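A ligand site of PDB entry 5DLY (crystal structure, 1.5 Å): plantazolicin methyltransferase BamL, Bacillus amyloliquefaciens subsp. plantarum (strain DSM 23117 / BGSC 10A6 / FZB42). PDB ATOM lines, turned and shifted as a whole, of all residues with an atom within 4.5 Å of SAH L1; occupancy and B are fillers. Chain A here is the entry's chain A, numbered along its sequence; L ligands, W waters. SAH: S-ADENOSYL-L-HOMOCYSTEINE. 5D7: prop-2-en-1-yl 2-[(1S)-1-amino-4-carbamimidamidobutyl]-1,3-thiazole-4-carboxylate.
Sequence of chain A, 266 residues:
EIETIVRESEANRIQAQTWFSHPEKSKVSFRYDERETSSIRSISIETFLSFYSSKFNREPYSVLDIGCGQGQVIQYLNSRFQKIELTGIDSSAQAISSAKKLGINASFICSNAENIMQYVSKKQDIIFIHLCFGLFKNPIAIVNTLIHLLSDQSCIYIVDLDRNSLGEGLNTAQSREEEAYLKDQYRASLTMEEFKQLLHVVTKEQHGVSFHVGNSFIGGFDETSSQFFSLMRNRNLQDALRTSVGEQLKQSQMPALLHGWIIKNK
OD1 of Asn 112 is in hydrogen-bond range of N6 of SAH L1.
The side-chain carboxylate of Asp 90 sits at hydrogen-bond distance from an oxygen (O2') of SAH L1 (2.6 Å).
The backbone carbonyl oxygen of His 130 sits at hydrogen-bond distance from a nitrogen (N) of SAH L1 (2.8 Å).
The backbone NH (N) of Ser 91 is in hydrogen-bond range of a nitrogen (N3) of SAH L1, 3.3 Å away.
O of Leu 131 sits at hydrogen-bond distance from N of 5D7 L2, 3.0 Å away.
A nitrogen (N) of 5D7 L2 lies within salt-bridge range of the side-chain carboxylate (OD2) of Asp 33.
A nitrogen (N) of SAH L1 sits at hydrogen-bond distance from the backbone carbonyl oxygen (O) of Gly 67.
The backbone NH of Ala 113 lies within hydrogen-bond range of a nitrogen (N1) of SAH L1 (2.9 Å).
Gln 17 touches SAH L1 (OE1 to C8, 3.1 Å).
Phe 20 touches SAH L1.
Gly 69 touches SAH L1.
Ser 92 touches SAH L1 (CB to O2', 3.7 Å).
Ser 111 touches SAH L1.
Cys 132 touches SAH L1.
Leu 135 touches SAH L1.
CE1 of Phe 136 touches C5 of SAH L1, at 3.6 Å.
Within 4 Å of SAH L1: Gln 17, Phe 20, Gly 67, Gly 69, Asp 90, Ser 91, Ser 92, Ser 111, Asn 112, Ala 113, His 130, Cys 132, Leu 135 and Phe 136.
The side-chain sulfur of Cys 132 sits at hydrogen-bond distance from the backbone carbonyl oxygen of Ile 66 (3.4 Å).
O of Ile 89 lies within hydrogen-bond range of N of Gly 67 (2.7 Å).
N of Gly 69 lies within hydrogen-bond range of OD2 of Asp 90.
The backbone carbonyl oxygen of His 130 lies within hydrogen-bond range of the side-chain sulfur of Cys 132, 3.8 Å away.
The backbone NH (N) of Ser 92 lies within hydrogen-bond range of the side-chain carboxylate (OD1) of Asp 90 (2.9 Å).
The backbone carbonyl oxygen (O) of Asp 90 is in hydrogen-bond range of the backbone NH (N) of Ser 111, 3.1 Å away.
Water W2 lies within hydrogen-bond range of O2' of SAH L1, OG of Ser 91, NE2 of Gln 17 and N of Ser 92.
Water W8 bridges N7 of SAH L1 (2.7 Å) and O of Leu 135 (2.9 Å).
Water W3 lies within hydrogen-bond range of O of Ile 66, N of His 130 and N of SAH L1.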
ATOM      1  N   GLN A  17      24.312 -10.136  15.683  1.00  0.00           N
ATOM      2  CA  GLN A  17      24.181 -10.693  14.350  1.00  0.00           C
ATOM      3  C   GLN A  17      24.131 -12.236  14.328  1.00  0.00           C
ATOM      4  O   GLN A  17      23.598 -12.821  13.385  1.00  0.00           O
ATOM      5  CB  GLN A  17      25.270 -10.120  13.421  1.00  0.00           C
ATOM      6  CG  GLN A  17      25.390 -10.770  12.038  1.00  0.00           C
ATOM      7  CD  GLN A  17      24.149 -10.678  11.183  1.00  0.00           C
ATOM      8  OE1 GLN A  17      23.234  -9.887  11.440  1.00  0.00           O
ATOM      9  NE2 GLN A  17      24.096 -11.517  10.152  1.00  0.00           N
ATOM     10  N   PHE A  20      20.871 -13.901  13.344  1.00  0.00           N
ATOM     11  CA  PHE A  20      20.439 -13.897  11.953  1.00  0.00           C
ATOM     12  C   PHE A  20      21.290 -14.810  11.069  1.00  0.00           C
ATOM     13  O   PHE A  20      20.969 -15.010   9.903  1.00  0.00           O
ATOM     14  CB  PHE A  20      20.377 -12.462  11.418  1.00  0.00           C
ATOM     15  CG  PHE A  20      19.409 -11.621  12.186  1.00  0.00           C
ATOM     16  CD1 PHE A  20      18.047 -11.674  11.891  1.00  0.00           C
ATOM     17  CD2 PHE A  20      19.832 -10.853  13.263  1.00  0.00           C
ATOM     18  CE1 PHE A  20      17.133 -10.954  12.628  1.00  0.00           C
ATOM     19  CE2 PHE A  20      18.922 -10.120  13.997  1.00  0.00           C
ATOM     20  CZ  PHE A  20      17.572 -10.167  13.676  1.00  0.00           C
ATOM     21  N   ASP A  33      10.303 -11.138  15.319  1.00  0.00           N
ATOM     22  CA  ASP A  33      10.257  -9.982  14.422  1.00  0.00           C
ATOM     23  C   ASP A  33       8.940  -9.899  13.666  1.00  0.00           C
ATOM     24  O   ASP A  33       8.368  -8.822  13.526  1.00  0.00           O
ATOM     25  CB  ASP A  33      11.420 -10.011  13.428  1.00  0.00           C
ATOM     26  CG  ASP A  33      12.781  -9.779  14.100  1.00  0.00           C
ATOM     27  OD1 ASP A  33      12.825  -9.492  15.320  1.00  0.00           O
ATOM     28  OD2 ASP A  33      13.791  -9.890  13.383  1.00  0.00           O
ATOM     29  N   ARG A  41       6.415  -1.766  10.051  1.00  0.00           N
ATOM     30  CA  ARG A  41       6.973  -1.741   8.702  1.00  0.00           C
ATOM     31  C   ARG A  41       6.261  -0.737   7.781  1.00  0.00           C
ATOM     32  O   ARG A  41       6.902   0.140   7.187  1.00  0.00           O
ATOM     33  CB  ARG A  41       6.935  -3.148   8.103  1.00  0.00           C
ATOM     34  CG  ARG A  41       8.132  -3.500   7.232  1.00  0.00           C
ATOM     35  CD  ARG A  41       8.513  -4.971   7.413  1.00  0.00           C
ATOM     36  NE  ARG A  41       7.375  -5.873   7.196  1.00  0.00           N
ATOM     37  CZ  ARG A  41       7.272  -7.109   7.686  1.00  0.00           C
ATOM     38  NH1 ARG A  41       8.239  -7.638   8.441  1.00  0.00           N
ATOM     39  NH2 ARG A  41       6.195  -7.823   7.417  1.00  0.00           N
ATOM     40  N   ILE A  66      18.245  -1.805   2.702  1.00  0.00           N
ATOM     41  CA  ILE A  66      19.471  -2.378   3.295  1.00  0.00           C
ATOM     42  C   ILE A  66      19.104  -3.363   4.406  1.00  0.00           C
ATOM     43  O   ILE A  66      18.392  -3.011   5.327  1.00  0.00           O
ATOM     44  CB  ILE A  66      20.394  -1.260   3.860  1.00  0.00           C
ATOM     45  CG1 ILE A  66      20.740  -0.202   2.782  1.00  0.00           C
ATOM     46  CG2 ILE A  66      21.650  -1.857   4.492  1.00  0.00           C
ATOM     47  CD1 ILE A  66      21.499  -0.713   1.573  1.00  0.00           C
ATOM     48  N   GLY A  67      19.595  -4.594   4.315  1.00  0.00           N
ATOM     49  CA  GLY A  67      19.189  -5.633   5.262  1.00  0.00           C
ATOM     50  C   GLY A  67      17.747  -6.011   5.023  1.00  0.00           C
ATOM     51  O   GLY A  67      16.923  -5.994   5.946  1.00  0.00           O
ATOM     52  N   GLY A  69      16.028  -8.641   4.480  1.00  0.00           N
ATOM     53  CA  GLY A  69      15.399  -9.870   4.967  1.00  0.00           C
ATOM     54  C   GLY A  69      14.776 -10.652   3.826  1.00  0.00           C
ATOM     55  O   GLY A  69      15.354 -10.733   2.750  1.00  0.00           O
ATOM     56  N   VAL A  73       9.513  -5.645   2.872  1.00  0.00           N
ATOM     57  CA  VAL A  73       9.436  -4.216   2.574  1.00  0.00           C
ATOM     58  C   VAL A  73       9.320  -3.977   1.069  1.00  0.00           C
ATOM     59  O   VAL A  73       8.530  -3.149   0.624  1.00  0.00           O
ATOM     60  CB  VAL A  73      10.632  -3.442   3.186  1.00  0.00           C
ATOM     61  CG1 VAL A  73      10.775  -2.051   2.562  1.00  0.00           C
ATOM     62  CG2 VAL A  73      10.471  -3.327   4.685  1.00  0.00           C
ATOM     63  N   ILE A  89      19.326  -5.732  -0.372  1.00  0.00           N
ATOM     64  CA  ILE A  89      20.589  -6.428  -0.086  1.00  0.00           C
ATOM     65  C   ILE A  89      20.566  -6.982   1.336  1.00  0.00           C
ATOM     66  O   ILE A  89      20.115  -6.327   2.278  1.00  0.00           O
ATOM     67  CB  ILE A  89      21.833  -5.522  -0.305  1.00  0.00           C
ATOM     68  CG1 ILE A  89      23.145  -6.313  -0.108  1.00  0.00           C
ATOM     69  CG2 ILE A  89      21.784  -4.290   0.592  1.00  0.00           C
ATOM     70  CD1 ILE A  89      24.361  -5.609  -0.674  1.00  0.00           C
ATOM     71  N   ASP A  90      21.036  -8.214   1.488  1.00  0.00           N
ATOM     72  CA  ASP A  90      21.068  -8.864   2.791  1.00  0.00           C
ATOM     73  C   ASP A  90      22.173  -9.889   2.761  1.00  0.00           C
ATOM     74  O   ASP A  90      22.404 -10.505   1.726  1.00  0.00           O
ATOM     75  CB  ASP A  90      19.722  -9.547   3.093  1.00  0.00           C
ATOM     76  CG  ASP A  90      19.527  -9.835   4.563  1.00  0.00           C
ATOM     77  OD1 ASP A  90      20.227 -10.715   5.100  1.00  0.00           O
ATOM     78  OD2 ASP A  90      18.667  -9.166   5.208  1.00  0.00           O
ATOM     79  N   SER A  91      22.886 -10.052   3.878  1.00  0.00           N
ATOM     80  CA  SER A  91      24.006 -11.010   3.934  1.00  0.00           C
ATOM     81  C   SER A  91      23.559 -12.453   4.210  1.00  0.00           C
ATOM     82  O   SER A  91      24.395 -13.364   4.228  1.00  0.00           O
ATOM     83  CB  SER A  91      25.047 -10.545   4.962  1.00  0.00           C
ATOM     84  OG  SER A  91      24.437 -10.405   6.228  1.00  0.00           O
ATOM     85  N   SER A  92      22.272 -12.657   4.436  1.00  0.00           N
ATOM     86  CA  SER A  92      21.726 -14.009   4.645  1.00  0.00           C
ATOM     87  C   SER A  92      21.271 -14.637   3.329  1.00  0.00           C
ATOM     88  O   SER A  92      20.324 -14.148   2.700  1.00  0.00           O
ATOM     89  CB  SER A  92      20.573 -13.990   5.640  1.00  0.00           C
ATOM     90  OG  SER A  92      19.875 -15.221   5.601  1.00  0.00           O
ATOM     91  N   SER A 111      24.984 -10.194  -0.052  1.00  0.00           N
ATOM     92  CA  SER A 111      26.312  -9.681   0.235  1.00  0.00           C
ATOM     93  C   SER A 111      26.225  -8.789   1.455  1.00  0.00           C
ATOM     94  O   SER A 111      25.140  -8.305   1.800  1.00  0.00           O
ATOM     95  CB  SER A 111      26.836  -8.875  -0.965  1.00  0.00           C
ATOM     96  OG  SER A 111      28.234  -8.607  -0.844  1.00  0.00           O
ATOM     97  N   ASN A 112      27.365  -8.584   2.113  1.00  0.00           N
ATOM     98  CA  ASN A 112      27.493  -7.539   3.117  1.00  0.00           C
ATOM     99  C   ASN A 112      27.122  -6.205   2.457  1.00  0.00           C
ATOM    100  O   ASN A 112      27.565  -5.907   1.340  1.00  0.00           O
ATOM    101  CB  ASN A 112      28.944  -7.546   3.610  1.00  0.00           C
ATOM    102  CG  ASN A 112      29.259  -6.500   4.670  1.00  0.00           C
ATOM    103  OD1 ASN A 112      28.417  -5.709   5.101  1.00  0.00           O
ATOM    104  ND2 ASN A 112      30.529  -6.488   5.066  1.00  0.00           N
ATOM    105  N   ALA A 113      26.286  -5.409   3.128  1.00  0.00           N
ATOM    106  CA  ALA A 113      25.889  -4.097   2.609  1.00  0.00           C
ATOM    107  C   ALA A 113      27.093  -3.201   2.323  1.00  0.00           C
ATOM    108  O   ALA A 113      27.002  -2.295   1.501  1.00  0.00           O
ATOM    109  CB  ALA A 113      24.932  -3.394   3.552  1.00  0.00           C
ATOM    110  N   HIS A 130      16.065  -0.377   7.937  1.00  0.00           N
ATOM    111  CA  HIS A 130      15.003  -0.569   8.918  1.00  0.00           C
ATOM    112  C   HIS A 130      15.340  -1.702   9.875  1.00  0.00           C
ATOM    113  O   HIS A 130      15.489  -2.856   9.483  1.00  0.00           O
ATOM    114  CB  HIS A 130      13.683  -0.853   8.172  1.00  0.00           C
ATOM    115  CG  HIS A 130      12.471  -0.841   9.054  1.00  0.00           C
ATOM    116  ND1 HIS A 130      11.912   0.303   9.560  1.00  0.00           N
ATOM    117  CD2 HIS A 130      11.676  -1.858   9.453  1.00  0.00           C
ATOM    118  CE1 HIS A 130      10.840  -0.011  10.277  1.00  0.00           C
ATOM    119  NE2 HIS A 130      10.674  -1.316  10.218  1.00  0.00           N
ATOM    120  N   LEU A 131      15.423  -1.338  11.154  1.00  0.00           N
ATOM    121  CA  LEU A 131      15.609  -2.298  12.248  1.00  0.00           C
ATOM    122  C   LEU A 131      16.811  -3.235  12.061  1.00  0.00           C
ATOM    123  O   LEU A 131      16.744  -4.446  12.368  1.00  0.00           O
ATOM    124  CB  LEU A 131      14.284  -3.038  12.561  1.00  0.00           C
ATOM    125  CG  LEU A 131      13.038  -2.173  12.806  1.00  0.00           C
ATOM    126  CD1 LEU A 131      11.798  -3.021  13.049  1.00  0.00           C
ATOM    127  CD2 LEU A 131      13.271  -1.209  13.969  1.00  0.00           C
ATOM    128  N   CYS A 132      17.926  -2.693  11.585  1.00  0.00           N
ATOM    129  CA  CYS A 132      19.126  -3.524  11.400  1.00  0.00           C
ATOM    130  C   CYS A 132      20.477  -2.838  11.574  1.00  0.00           C
ATOM    131  O   CYS A 132      21.508  -3.516  11.513  1.00  0.00           O
ATOM    132  CB  CYS A 132      19.102  -4.239  10.042  1.00  0.00           C
ATOM    133  SG  CYS A 132      19.129  -3.171   8.593  1.00  0.00           S
ATOM    134  N   LEU A 135      23.306  -4.204  13.744  1.00  0.00           N
ATOM    135  CA  LEU A 135      23.878  -5.511  13.376  1.00  0.00           C
ATOM    136  C   LEU A 135      25.168  -5.386  12.569  1.00  0.00           C
ATOM    137  O   LEU A 135      25.920  -6.357  12.474  1.00  0.00           O
ATOM    138  CB  LEU A 135      22.875  -6.349  12.563  1.00  0.00           C
ATOM    139  CG  LEU A 135      21.547  -6.666  13.256  1.00  0.00           C
ATOM    140  CD1 LEU A 135      20.612  -7.356  12.281  1.00  0.00           C
ATOM    141  CD2 LEU A 135      21.836  -7.560  14.450  1.00  0.00           C
ATOM    142  N   PHE A 136      25.410  -4.220  11.987  1.00  0.00           N
ATOM    143  CA  PHE A 136      26.535  -4.054  11.074  1.00  0.00           C
ATOM    144  C   PHE A 136      27.855  -3.987  11.828  1.00  0.00           C
ATOM    145  O   PHE A 136      27.975  -3.243  12.793  1.00  0.00           O
ATOM    146  CB  PHE A 136      26.381  -2.787  10.229  1.00  0.00           C
ATOM    147  CG  PHE A 136      25.107  -2.718   9.433  1.00  0.00           C
ATOM    148  CD1 PHE A 136      24.433  -3.874   9.036  1.00  0.00           C
ATOM    149  CD2 PHE A 136      24.589  -1.489   9.054  1.00  0.00           C
ATOM    150  CE1 PHE A 136      23.250  -3.796   8.305  1.00  0.00           C
ATOM    151  CE2 PHE A 136      23.423  -1.398   8.302  1.00  0.00           C
ATOM    152  CZ  PHE A 136      22.758  -2.551   7.933  1.00  0.00           C
HETATM  153  N   SAH L   1      15.036  -4.530   7.306  1.00  0.00           N
HETATM  154  CA  SAH L   1      14.430  -5.728   7.969  1.00  0.00           C
HETATM  155  CB  SAH L   1      15.368  -6.251   9.060  1.00  0.00           C
HETATM  156  CG  SAH L   1      15.411  -7.782   9.049  1.00  0.00           C
HETATM  157  SD  SAH L   1      16.275  -8.435  10.446  1.00  0.00           S
HETATM  158  C   SAH L   1      13.105  -5.363   8.584  1.00  0.00           C
HETATM  159  O   SAH L   1      12.575  -4.280   8.353  1.00  0.00           O
HETATM  160  OXT SAH L   1      12.511  -6.130   9.336  1.00  0.00           O
HETATM  161  C5' SAH L   1      17.938  -7.886  10.175  1.00  0.00           C
HETATM  162  C4' SAH L   1      18.478  -8.268   8.802  1.00  0.00           C
HETATM  163  O4' SAH L   1      19.725  -7.597   8.589  1.00  0.00           O
HETATM  164  C3' SAH L   1      18.770  -9.757   8.672  1.00  0.00           C
HETATM  165  O3' SAH L   1      18.048 -10.314   7.560  1.00  0.00           O
HETATM  166  C2' SAH L   1      20.293  -9.832   8.491  1.00  0.00           C
HETATM  167  O2' SAH L   1      20.746 -10.903   7.650  1.00  0.00           O
HETATM  168  C1' SAH L   1      20.577  -8.483   7.870  1.00  0.00           C
HETATM  169  N9  SAH L   1      21.981  -8.025   7.970  1.00  0.00           N
HETATM  170  C8  SAH L   1      22.748  -8.018   9.073  1.00  0.00           C
HETATM  171  N7  SAH L   1      23.980  -7.530   8.792  1.00  0.00           N
HETATM  172  C5  SAH L   1      24.001  -7.205   7.493  1.00  0.00           C
HETATM  173  C6  SAH L   1      24.998  -6.641   6.569  1.00  0.00           C
HETATM  174  N6  SAH L   1      26.213  -6.324   7.042  1.00  0.00           N
HETATM  175  N1  SAH L   1      24.620  -6.450   5.280  1.00  0.00           N
HETATM  176  C2  SAH L   1      23.383  -6.782   4.840  1.00  0.00           C
HETATM  177  N3  SAH L   1      22.416  -7.308   5.637  1.00  0.00           N
HETATM  178  C4  SAH L   1      22.674  -7.540   6.952  1.00  0.00           C
HETATM  179  O9  5D7 L   2      11.966  -3.306  16.483  1.00  0.00           O
HETATM  180  C6  5D7 L   2      12.189  -4.127  17.358  1.00  0.00           C
HETATM  181  O7  5D7 L   2      11.484  -4.090  18.614  1.00  0.00           O
HETATM  182  C8  5D7 L   2      10.594  -3.025  18.950  1.00  0.00           C
HETATM  183  C2  5D7 L   2      13.172  -5.228  17.155  1.00  0.00           C
HETATM  184  N3  5D7 L   2      13.726  -5.483  15.939  1.00  0.00           N
HETATM  185  C4  5D7 L   2      14.584  -6.509  15.914  1.00  0.00           C
HETATM  186  S5  5D7 L   2      14.682  -7.207  17.501  1.00  0.00           S
HETATM  187  C1  5D7 L   2      13.564  -6.087  18.196  1.00  0.00           C
HETATM  188  CA  5D7 L   2      15.371  -7.076  14.798  1.00  0.00           C
HETATM  189  N   5D7 L   2      14.896  -6.467  13.563  1.00  0.00           N
HETATM  190  CB  5D7 L   2      16.881  -6.859  14.977  1.00  0.00           C
HETATM  191  CG  5D7 L   2      17.297  -5.462  15.467  1.00  0.00           C
HETATM  192  CD  5D7 L   2      18.675  -5.144  14.913  1.00  0.00           C
HETATM  193  NE  5D7 L   2      19.130  -3.883  15.487  1.00  0.00           N
HETATM  194  CZ  5D7 L   2      19.789  -3.678  16.626  1.00  0.00           C
HETATM  195  NH2 5D7 L   2      20.106  -2.507  16.977  1.00  0.00           N
HETATM  196  NH1 5D7 L   2      20.132  -4.662  17.370  1.00  0.00           N
HETATM  197  C3  5D7 L   2      10.086  -3.250  20.350  1.00  0.00           C
HETATM  198  C5  5D7 L   2       8.865  -2.898  20.697  1.00  0.00           C
HETATM  199  O   HOH W   1      12.538  -8.386   6.808  1.00  0.00           O
HETATM  200  O   HOH W   2      23.043 -12.131   7.645  1.00  0.00           O
HETATM  201  O   HOH W   3      15.843  -2.090   5.793  1.00  0.00           O
HETATM  202  O   HOH W   4      10.016  -5.037  10.367  1.00  0.00           O
HETATM  203  O   HOH W   5      28.444  -6.678   9.186  1.00  0.00           O
HETATM  204  O   HOH W   6      17.178 -12.634   7.860  1.00  0.00           O
HETATM  205  O   HOH W   7      13.530  -4.333   5.062  1.00  0.00           O
HETATM  206  O   HOH W   8      26.331  -8.004  10.088  1.00  0.00           O
